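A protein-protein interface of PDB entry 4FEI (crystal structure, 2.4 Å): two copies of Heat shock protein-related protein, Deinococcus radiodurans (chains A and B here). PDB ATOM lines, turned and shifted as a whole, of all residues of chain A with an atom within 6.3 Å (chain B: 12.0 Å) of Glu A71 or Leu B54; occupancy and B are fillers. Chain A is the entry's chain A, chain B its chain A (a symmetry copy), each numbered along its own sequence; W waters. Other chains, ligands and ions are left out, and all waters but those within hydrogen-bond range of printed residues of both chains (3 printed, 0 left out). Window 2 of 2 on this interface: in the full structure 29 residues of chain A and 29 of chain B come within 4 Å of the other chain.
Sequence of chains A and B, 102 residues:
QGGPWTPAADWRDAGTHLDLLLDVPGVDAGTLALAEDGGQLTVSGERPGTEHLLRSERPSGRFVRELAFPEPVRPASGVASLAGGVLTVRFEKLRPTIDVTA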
ATOM      1  N   TRP A  11     -25.182 -25.503  -1.572  1.00  0.00           N
ATOM      2  CA  TRP A  11     -24.079 -24.696  -2.071  1.00  0.00           C
ATOM      3  C   TRP A  11     -24.580 -23.294  -2.406  1.00  0.00           C
ATOM      4  O   TRP A  11     -25.487 -23.112  -3.201  1.00  0.00           O
ATOM      5  CB  TRP A  11     -23.474 -25.338  -3.312  1.00  0.00           C
ATOM      6  CG  TRP A  11     -22.657 -26.586  -2.971  1.00  0.00           C
ATOM      7  CD1 TRP A  11     -23.046 -27.893  -3.125  1.00  0.00           C
ATOM      8  CD2 TRP A  11     -21.317 -26.619  -2.447  1.00  0.00           C
ATOM      9  NE1 TRP A  11     -22.018 -28.740  -2.703  1.00  0.00           N
ATOM     10  CE2 TRP A  11     -20.958 -27.981  -2.275  1.00  0.00           C
ATOM     11  CE3 TRP A  11     -20.388 -25.637  -2.118  1.00  0.00           C
ATOM     12  CZ2 TRP A  11     -19.696 -28.378  -1.807  1.00  0.00           C
ATOM     13  CZ3 TRP A  11     -19.134 -26.026  -1.618  1.00  0.00           C
ATOM     14  CH2 TRP A  11     -18.805 -27.382  -1.466  1.00  0.00           C
ATOM     15  N   ARG A  12     -24.009 -22.303  -1.745  1.00  0.00           N
ATOM     16  CA  ARG A  12     -24.402 -20.911  -1.981  1.00  0.00           C
ATOM     17  C   ARG A  12     -23.273 -20.186  -2.719  1.00  0.00           C
ATOM     18  O   ARG A  12     -22.089 -20.341  -2.391  1.00  0.00           O
ATOM     19  CB  ARG A  12     -24.727 -20.212  -0.652  1.00  0.00           C
ATOM     20  CG  ARG A  12     -25.013 -18.695  -0.769  1.00  0.00           C
ATOM     21  CD  ARG A  12     -25.295 -18.088   0.603  1.00  0.00           C
ATOM     22  NE  ARG A  12     -24.222 -18.311   1.598  1.00  0.00           N
ATOM     23  CZ  ARG A  12     -24.396 -18.251   2.925  1.00  0.00           C
ATOM     24  NH1 ARG A  12     -25.619 -18.001   3.439  1.00  0.00           N
ATOM     25  NH2 ARG A  12     -23.356 -18.462   3.749  1.00  0.00           N
ATOM     26  N   ASP A  13     -23.660 -19.434  -3.740  1.00  0.00           N
ATOM     27  CA  ASP A  13     -22.744 -18.618  -4.479  1.00  0.00           C
ATOM     28  C   ASP A  13     -22.599 -17.342  -3.682  1.00  0.00           C
ATOM     29  O   ASP A  13     -23.526 -16.557  -3.601  1.00  0.00           O
ATOM     30  CB  ASP A  13     -23.339 -18.344  -5.861  1.00  0.00           C
ATOM     31  CG  ASP A  13     -22.495 -17.402  -6.705  1.00  0.00           C
ATOM     32  OD1 ASP A  13     -21.323 -17.129  -6.346  1.00  0.00           O
ATOM     33  OD2 ASP A  13     -23.030 -16.922  -7.744  1.00  0.00           O
ATOM     34  N   LEU A  18     -17.361 -19.627  -2.294  1.00  0.00           N
ATOM     35  CA  LEU A  18     -18.348 -20.688  -2.448  1.00  0.00           C
ATOM     36  C   LEU A  18     -18.629 -21.234  -1.037  1.00  0.00           C
ATOM     37  O   LEU A  18     -17.697 -21.667  -0.340  1.00  0.00           O
ATOM     38  CB  LEU A  18     -17.750 -21.775  -3.337  1.00  0.00           C
ATOM     39  CG  LEU A  18     -18.623 -22.921  -3.820  1.00  0.00           C
ATOM     40  CD1 LEU A  18     -19.828 -22.409  -4.660  1.00  0.00           C
ATOM     41  CD2 LEU A  18     -17.774 -23.888  -4.635  1.00  0.00           C
ATOM     42  N   ALA A  68     -19.160 -32.826  -4.388  1.00  0.00           N
ATOM     43  CA  ALA A  68     -18.332 -32.252  -5.470  1.00  0.00           C
ATOM     44  C   ALA A  68     -18.545 -30.769  -5.480  1.00  0.00           C
ATOM     45  O   ALA A  68     -19.703 -30.319  -5.341  1.00  0.00           O
ATOM     46  CB  ALA A  68     -18.752 -32.834  -6.825  1.00  0.00           C
ATOM     47  N   PHE A  69     -17.465 -29.998  -5.619  1.00  0.00           N
ATOM     48  CA  PHE A  69     -17.592 -28.526  -5.757  1.00  0.00           C
ATOM     49  C   PHE A  69     -18.342 -28.166  -7.047  1.00  0.00           C
ATOM     50  O   PHE A  69     -17.976 -28.625  -8.113  1.00  0.00           O
ATOM     51  CB  PHE A  69     -16.232 -27.838  -5.779  1.00  0.00           C
ATOM     52  CG  PHE A  69     -15.446 -27.987  -4.512  1.00  0.00           C
ATOM     53  CD1 PHE A  69     -14.275 -28.769  -4.476  1.00  0.00           C
ATOM     54  CD2 PHE A  69     -15.849 -27.329  -3.361  1.00  0.00           C
ATOM     55  CE1 PHE A  69     -13.548 -28.909  -3.295  1.00  0.00           C
ATOM     56  CE2 PHE A  69     -15.120 -27.450  -2.160  1.00  0.00           C
ATOM     57  CZ  PHE A  69     -13.964 -28.240  -2.131  1.00  0.00           C
ATOM     58  N   PRO A  70     -19.391 -27.340  -6.941  1.00  0.00           N
ATOM     59  CA  PRO A  70     -20.161 -26.900  -8.133  1.00  0.00           C
ATOM     60  C   PRO A  70     -19.326 -25.975  -8.990  1.00  0.00           C
ATOM     61  O   PRO A  70     -19.629 -25.789 -10.171  1.00  0.00           O
ATOM     62  CB  PRO A  70     -21.349 -26.089  -7.530  1.00  0.00           C
ATOM     63  CG  PRO A  70     -21.385 -26.482  -6.066  1.00  0.00           C
ATOM     64  CD  PRO A  70     -19.960 -26.813  -5.683  1.00  0.00           C
ATOM     65  N   GLU A  71     -18.296 -25.389  -8.367  1.00  0.00           N
ATOM     66  CA  GLU A  71     -17.401 -24.412  -8.991  1.00  0.00           C
ATOM     67  C   GLU A  71     -15.990 -24.719  -8.494  1.00  0.00           C
ATOM     68  O   GLU A  71     -15.819 -24.998  -7.314  1.00  0.00           O
ATOM     69  CB  GLU A  71     -17.803 -23.025  -8.505  1.00  0.00           C
ATOM     70  CG  GLU A  71     -17.862 -21.977  -9.557  1.00  0.00           C
ATOM     71  CD  GLU A  71     -19.139 -22.082 -10.376  1.00  0.00           C
ATOM     72  OE1 GLU A  71     -19.139 -22.890 -11.361  1.00  0.00           O
ATOM     73  OE2 GLU A  71     -20.121 -21.335 -10.045  1.00  0.00           O
ATOM     74  N   PRO A  72     -14.971 -24.647  -9.380  1.00  0.00           N
ATOM     75  CA  PRO A  72     -13.582 -24.835  -8.924  1.00  0.00           C
ATOM     76  C   PRO A  72     -13.155 -23.804  -7.859  1.00  0.00           C
ATOM     77  O   PRO A  72     -13.466 -22.626  -7.975  1.00  0.00           O
ATOM     78  CB  PRO A  72     -12.759 -24.716 -10.213  1.00  0.00           C
ATOM     79  CG  PRO A  72     -13.696 -23.999 -11.199  1.00  0.00           C
ATOM     80  CD  PRO A  72     -15.058 -24.460 -10.844  1.00  0.00           C
ATOM     81  N   VAL A  73     -12.462 -24.268  -6.821  1.00  0.00           N
ATOM     82  CA  VAL A  73     -12.000 -23.398  -5.736  1.00  0.00           C
ATOM     83  C   VAL A  73     -10.480 -23.411  -5.608  1.00  0.00           C
ATOM     84  O   VAL A  73      -9.829 -24.360  -6.048  1.00  0.00           O
ATOM     85  CB  VAL A  73     -12.640 -23.770  -4.358  1.00  0.00           C
ATOM     86  CG1 VAL A  73     -14.176 -23.663  -4.412  1.00  0.00           C
ATOM     87  CG2 VAL A  73     -12.213 -25.173  -3.904  1.00  0.00           C
ATOM     88  N   LYS A  93     -13.301 -18.982  -4.568  1.00  0.00           N
ATOM     89  CA  LYS A  93     -13.388 -19.443  -5.946  1.00  0.00           C
ATOM     90  C   LYS A  93     -12.125 -19.103  -6.732  1.00  0.00           C
ATOM     91  O   LYS A  93     -11.434 -18.124  -6.462  1.00  0.00           O
ATOM     92  CB  LYS A  93     -14.615 -18.828  -6.626  1.00  0.00           C
ATOM     93  CG  LYS A  93     -15.925 -19.511  -6.236  1.00  0.00           C
ATOM     94  CD  LYS A  93     -17.136 -18.578  -6.267  1.00  0.00           C
ATOM     95  CE  LYS A  93     -17.615 -18.286  -7.661  1.00  0.00           C
ATOM     96  NZ  LYS A  93     -18.986 -17.622  -7.568  1.00  0.00           N
ATOM     97  N   ARG A  95     -12.334 -18.498 -10.031  1.00  0.00           N
ATOM     98  CA  ARG A  95     -12.857 -17.456 -10.866  1.00  0.00           C
ATOM     99  C   ARG A  95     -13.969 -16.764 -10.049  1.00  0.00           C
ATOM    100  O   ARG A  95     -15.157 -17.135 -10.137  1.00  0.00           O
ATOM    101  CB  ARG A  95     -13.394 -18.061 -12.171  1.00  0.00           C
ATOM    102  CG  ARG A  95     -13.977 -17.065 -13.196  1.00  0.00           C
ATOM    103  CD  ARG A  95     -14.568 -17.832 -14.416  1.00  0.00           C
ATOM    104  NE  ARG A  95     -15.638 -17.079 -15.090  1.00  0.00           N
ATOM    105  CZ  ARG A  95     -16.918 -17.011 -14.671  1.00  0.00           C
ATOM    106  NH1 ARG A  95     -17.808 -16.287 -15.361  1.00  0.00           N
ATOM    107  NH2 ARG A  95     -17.322 -17.658 -13.565  1.00  0.00           N
ATOM    108  N   GLN B   1     -35.975 -25.153  -5.653  1.00  0.00           N
ATOM    109  CA  GLN B   1     -34.739 -24.895  -4.841  1.00  0.00           C
ATOM    110  C   GLN B   1     -35.116 -24.317  -3.483  1.00  0.00           C
ATOM    111  O   GLN B   1     -35.630 -23.176  -3.422  1.00  0.00           O
ATOM    112  CB  GLN B   1     -33.795 -23.973  -5.607  1.00  0.00           C
ATOM    113  CG  GLN B   1     -33.166 -24.690  -6.799  1.00  0.00           C
ATOM    114  CD  GLN B   1     -32.965 -23.797  -8.035  1.00  0.00           C
ATOM    115  OE1 GLN B   1     -31.826 -23.562  -8.471  1.00  0.00           O
ATOM    116  NE2 GLN B   1     -34.070 -23.320  -8.620  1.00  0.00           N
ATOM    117  N   GLY B   2     -34.872 -25.108  -2.421  1.00  0.00           N
ATOM    118  CA  GLY B   2     -35.294 -24.829  -1.037  1.00  0.00           C
ATOM    119  C   GLY B   2     -36.682 -25.412  -0.713  1.00  0.00           C
ATOM    120  O   GLY B   2     -37.700 -24.732  -0.904  1.00  0.00           O
ATOM    121  N   GLY B  49     -34.803 -18.656   3.625  1.00  0.00           N
ATOM    122  CA  GLY B  49     -34.226 -19.329   2.479  1.00  0.00           C
ATOM    123  C   GLY B  49     -32.802 -18.855   2.238  1.00  0.00           C
ATOM    124  O   GLY B  49     -32.458 -17.679   2.418  1.00  0.00           O
ATOM    125  N   THR B  50     -31.958 -19.758   1.782  1.00  0.00           N
ATOM    126  CA  THR B  50     -30.564 -19.396   1.488  1.00  0.00           C
ATOM    127  C   THR B  50     -30.477 -18.684   0.151  1.00  0.00           C
ATOM    128  O   THR B  50     -31.108 -19.123  -0.829  1.00  0.00           O
ATOM    129  CB  THR B  50     -29.699 -20.640   1.522  1.00  0.00           C
ATOM    130  OG1 THR B  50     -30.009 -21.368   2.718  1.00  0.00           O
ATOM    131  CG2 THR B  50     -28.252 -20.289   1.536  1.00  0.00           C
ATOM    132  N   GLU B  51     -29.740 -17.575   0.112  1.00  0.00           N
ATOM    133  CA  GLU B  51     -29.657 -16.754  -1.109  1.00  0.00           C
ATOM    134  C   GLU B  51     -28.691 -17.361  -2.122  1.00  0.00           C
ATOM    135  O   GLU B  51     -27.786 -18.089  -1.737  1.00  0.00           O
ATOM    136  CB  GLU B  51     -29.210 -15.321  -0.779  1.00  0.00           C
ATOM    137  CG  GLU B  51     -30.189 -14.531   0.102  1.00  0.00           C
ATOM    138  CD  GLU B  51     -31.335 -13.861  -0.692  1.00  0.00           C
ATOM    139  OE1 GLU B  51     -32.511 -14.166  -0.383  1.00  0.00           O
ATOM    140  OE2 GLU B  51     -31.051 -13.038  -1.621  1.00  0.00           O
ATOM    141  N   HIS B  52     -28.894 -17.070  -3.406  1.00  0.00           N
ATOM    142  CA  HIS B  52     -27.956 -17.450  -4.492  1.00  0.00           C
ATOM    143  C   HIS B  52     -27.517 -18.915  -4.498  1.00  0.00           C
ATOM    144  O   HIS B  52     -26.319 -19.237  -4.524  1.00  0.00           O
ATOM    145  CB  HIS B  52     -26.740 -16.520  -4.503  1.00  0.00           C
ATOM    146  CG  HIS B  52     -27.092 -15.063  -4.550  1.00  0.00           C
ATOM    147  ND1 HIS B  52     -27.186 -14.352  -5.731  1.00  0.00           N
ATOM    148  CD2 HIS B  52     -27.349 -14.179  -3.559  1.00  0.00           C
ATOM    149  CE1 HIS B  52     -27.492 -13.095  -5.466  1.00  0.00           C
ATOM    150  NE2 HIS B  52     -27.607 -12.969  -4.154  1.00  0.00           N
ATOM    151  N   LEU B  53     -28.509 -19.796  -4.477  1.00  0.00           N
ATOM    152  CA  LEU B  53     -28.288 -21.241  -4.395  1.00  0.00           C
ATOM    153  C   LEU B  53     -27.787 -21.826  -5.720  1.00  0.00           C
ATOM    154  O   LEU B  53     -28.336 -21.555  -6.773  1.00  0.00           O
ATOM    155  CB  LEU B  53     -29.591 -21.926  -3.967  1.00  0.00           C
ATOM    156  CG  LEU B  53     -29.776 -22.573  -2.590  1.00  0.00           C
ATOM    157  CD1 LEU B  53     -28.820 -22.079  -1.515  1.00  0.00           C
ATOM    158  CD2 LEU B  53     -31.226 -22.387  -2.182  1.00  0.00           C
ATOM    159  N   LEU B  54     -26.749 -22.640  -5.640  1.00  0.00           N
ATOM    160  CA  LEU B  54     -26.208 -23.362  -6.783  1.00  0.00           C
ATOM    161  C   LEU B  54     -26.717 -24.792  -6.815  1.00  0.00           C
ATOM    162  O   LEU B  54     -27.035 -25.317  -7.899  1.00  0.00           O
ATOM    163  CB  LEU B  54     -24.693 -23.322  -6.747  1.00  0.00           C
ATOM    164  CG  LEU B  54     -23.886 -22.338  -7.626  1.00  0.00           C
ATOM    165  CD1 LEU B  54     -24.570 -21.077  -8.098  1.00  0.00           C
ATOM    166  CD2 LEU B  54     -22.532 -22.037  -6.932  1.00  0.00           C
ATOM    167  N   ARG B  55     -26.797 -25.403  -5.633  1.00  0.00           N
ATOM    168  CA  ARG B  55     -27.439 -26.700  -5.416  1.00  0.00           C
ATOM    169  C   ARG B  55     -28.198 -26.617  -4.115  1.00  0.00           C
ATOM    170  O   ARG B  55     -27.683 -26.046  -3.151  1.00  0.00           O
ATOM    171  CB  ARG B  55     -26.406 -27.815  -5.231  1.00  0.00           C
ATOM    172  CG  ARG B  55     -25.773 -28.327  -6.463  1.00  0.00           C
ATOM    173  CD  ARG B  55     -25.111 -29.675  -6.165  1.00  0.00           C
ATOM    174  NE  ARG B  55     -24.088 -29.933  -7.186  1.00  0.00           N
ATOM    175  CZ  ARG B  55     -22.819 -30.203  -6.919  1.00  0.00           C
ATOM    176  NH1 ARG B  55     -22.400 -30.286  -5.654  1.00  0.00           N
ATOM    177  NH2 ARG B  55     -21.989 -30.425  -7.912  1.00  0.00           N
ATOM    178  N   SER B  56     -29.353 -27.265  -4.036  1.00  0.00           N
ATOM    179  CA  SER B  56     -30.140 -27.222  -2.795  1.00  0.00           C
ATOM    180  C   SER B  56     -30.680 -28.599  -2.400  1.00  0.00           C
ATOM    181  O   SER B  56     -31.322 -29.272  -3.221  1.00  0.00           O
ATOM    182  CB  SER B  56     -31.303 -26.224  -2.966  1.00  0.00           C
ATOM    183  OG  SER B  56     -32.042 -26.075  -1.778  1.00  0.00           O
ATOM    184  N   GLU B  57     -30.426 -29.015  -1.156  1.00  0.00           N
ATOM    185  CA  GLU B  57     -31.106 -30.186  -0.546  1.00  0.00           C
ATOM    186  C   GLU B  57     -31.896 -29.751   0.709  1.00  0.00           C
ATOM    187  O   GLU B  57     -32.872 -30.420   1.118  1.00  0.00           O
ATOM    188  CB  GLU B  57     -30.093 -31.256  -0.126  1.00  0.00           C
ATOM    189  CG  GLU B  57     -29.298 -31.892  -1.237  1.00  0.00           C
ATOM    190  CD  GLU B  57     -28.196 -32.820  -0.692  1.00  0.00           C
ATOM    191  OE1 GLU B  57     -28.174 -33.063   0.537  1.00  0.00           O
ATOM    192  OE2 GLU B  57     -27.335 -33.312  -1.486  1.00  0.00           O
ATOM    193  N   ARG B  58     -31.485 -28.629   1.299  1.00  0.00           N
ATOM    194  CA  ARG B  58     -31.973 -28.205   2.596  1.00  0.00           C
ATOM    195  C   ARG B  58     -33.335 -27.550   2.498  1.00  0.00           C
ATOM    196  O   ARG B  58     -33.566 -26.741   1.594  1.00  0.00           O
ATOM    197  CB  ARG B  58     -30.991 -27.212   3.219  1.00  0.00           C
ATOM    198  CG  ARG B  58     -29.560 -27.775   3.512  1.00  0.00           C
ATOM    199  CD  ARG B  58     -28.858 -26.925   4.543  1.00  0.00           C
ATOM    200  NE  ARG B  58     -29.069 -25.515   4.220  1.00  0.00           N
ATOM    201  CZ  ARG B  58     -29.068 -24.516   5.099  1.00  0.00           C
ATOM    202  NH1 ARG B  58     -29.274 -23.275   4.665  1.00  0.00           N
ATOM    203  NH2 ARG B  58     -28.856 -24.748   6.395  1.00  0.00           N
ATOM    204  N   SER B  60     -36.464 -24.918   3.566  1.00  0.00           N
ATOM    205  CA  SER B  60     -36.540 -23.505   3.958  1.00  0.00           C
ATOM    206  C   SER B  60     -37.955 -23.126   4.338  1.00  0.00           C
ATOM    207  O   SER B  60     -38.901 -23.810   3.966  1.00  0.00           O
ATOM    208  CB  SER B  60     -36.188 -22.586   2.768  1.00  0.00           C
ATOM    209  OG  SER B  60     -34.819 -22.649   2.530  1.00  0.00           O
HETATM  210  O   HOH W   1     -28.009 -16.574   2.196  1.00  0.00           O
HETATM  211  O   HOH W   2     -23.728 -31.464  -2.694  1.00  0.00           O
HETATM  212  O   HOH W   3     -25.047 -14.724  -7.291  1.00  0.00           O
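N of Leu B54 is in hydrogen-bond range of O of Trp A11, 2.8 Å away. N of Trp A11 sits at hydrogen-bond distance from O of Arg B55 (3.0 Å). The backbone carbonyl oxygen of His B52 lies within hydrogen-bond range of the backbone NH of Asp A13 (2.8 Å). O of Ala A68 lies within hydrogen-bond range of NH1 of Arg B55, at 2.7 Å.
The side-chain carboxylate (OD1) of Asp A13 is in salt-bridge range of the side-chain amino group (NZ) of Lys A93, at 2.7 Å. OG1 of Thr B50 sits at hydrogen-bond distance from NH1 of Arg B58, 2.8 Å away.
Water W3 lies within hydrogen-bond range of ND1 of His B52 (2.7 Å) and OD2 of Asp A13 (3.0 Å). Water W1 lies within hydrogen-bond range of the backbone NH (N) of Glu B51 (2.9 Å) and the guanidinium group (NH1) of Arg A12 (3.0 Å). Water W2 lies within hydrogen-bond range of NE1 of Trp A11 (3.2 Å) and NH1 of Arg B55 (3.5 Å).
Trp A11 touches just these residues of chain B: Leu B53 (3.6 Å), Leu B54 (2.8 Å) and Arg B55 (3.0 Å). Of the printed residues of chain B, Asp A13 touches His B52 and Leu B54. No residue of chain B comes within 4 Å of Phe A69. Of chain B, only Arg B55 comes within 4 Å of Pro A70. Printed residues of chain B within 4 Å of Glu A71: Leu B54 (3.9996 Å). No residue of chain B comes within 4 Å of Pro A72. Lys A93 touches none of the printed residues of chain B. No residue of chain B comes within 4 Å of Arg A95. Of the printed residues of chain A, Thr B50 touches Arg A12 (3.8 Å). Printed residues of chain A within 4 Å of His B52: Arg A12 and Asp A13. Of the printed residues of chain A, Leu B53 touches Trp A11 (3.6 Å). Of the printed residues of chain A, Leu B54 touches Trp A11, Asp A13, Leu A18 and Glu A71. Ser B56 touches none of the printed residues of chain A. The nearest printed residue of chain B that does not touch Glu A71 is Arg B55 (6.3 Å). The nearest printed residue of chain A that does not touch Leu B54 is Pro A70 (4.3 Å).
No position is printed for both chains. Of the 12 pairs that touch across the chains among the printed residues, none has its exchanged pair printed and touching as well.
Trp A11 touches Leu B53. Arg A12 touches Thr B50. CG of Arg A12 touches O of Glu B51, 3.0 Å away. Arg A12 touches His B52. Asp A13 touches Leu B54. CD1 of Leu A18 touches CD2 of Leu B54, at 3.6 Å. Pro A70 touches Arg B55 (CG to NH1, 3.96 Å). Leu B54 touches Glu A71 (CD2 to OE2, 3.9996 Å).
Hydrophobic or aromatic side chains of chain A within 4 Å of the printed part of chain B: Trp A11, Leu A18 and Pro A70. Along chain A the printed residues that touch a printed residue of chain B span positions 11 to 71. Of the 13 printed residues of chain B, 6 touch a printed residue of chain A.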
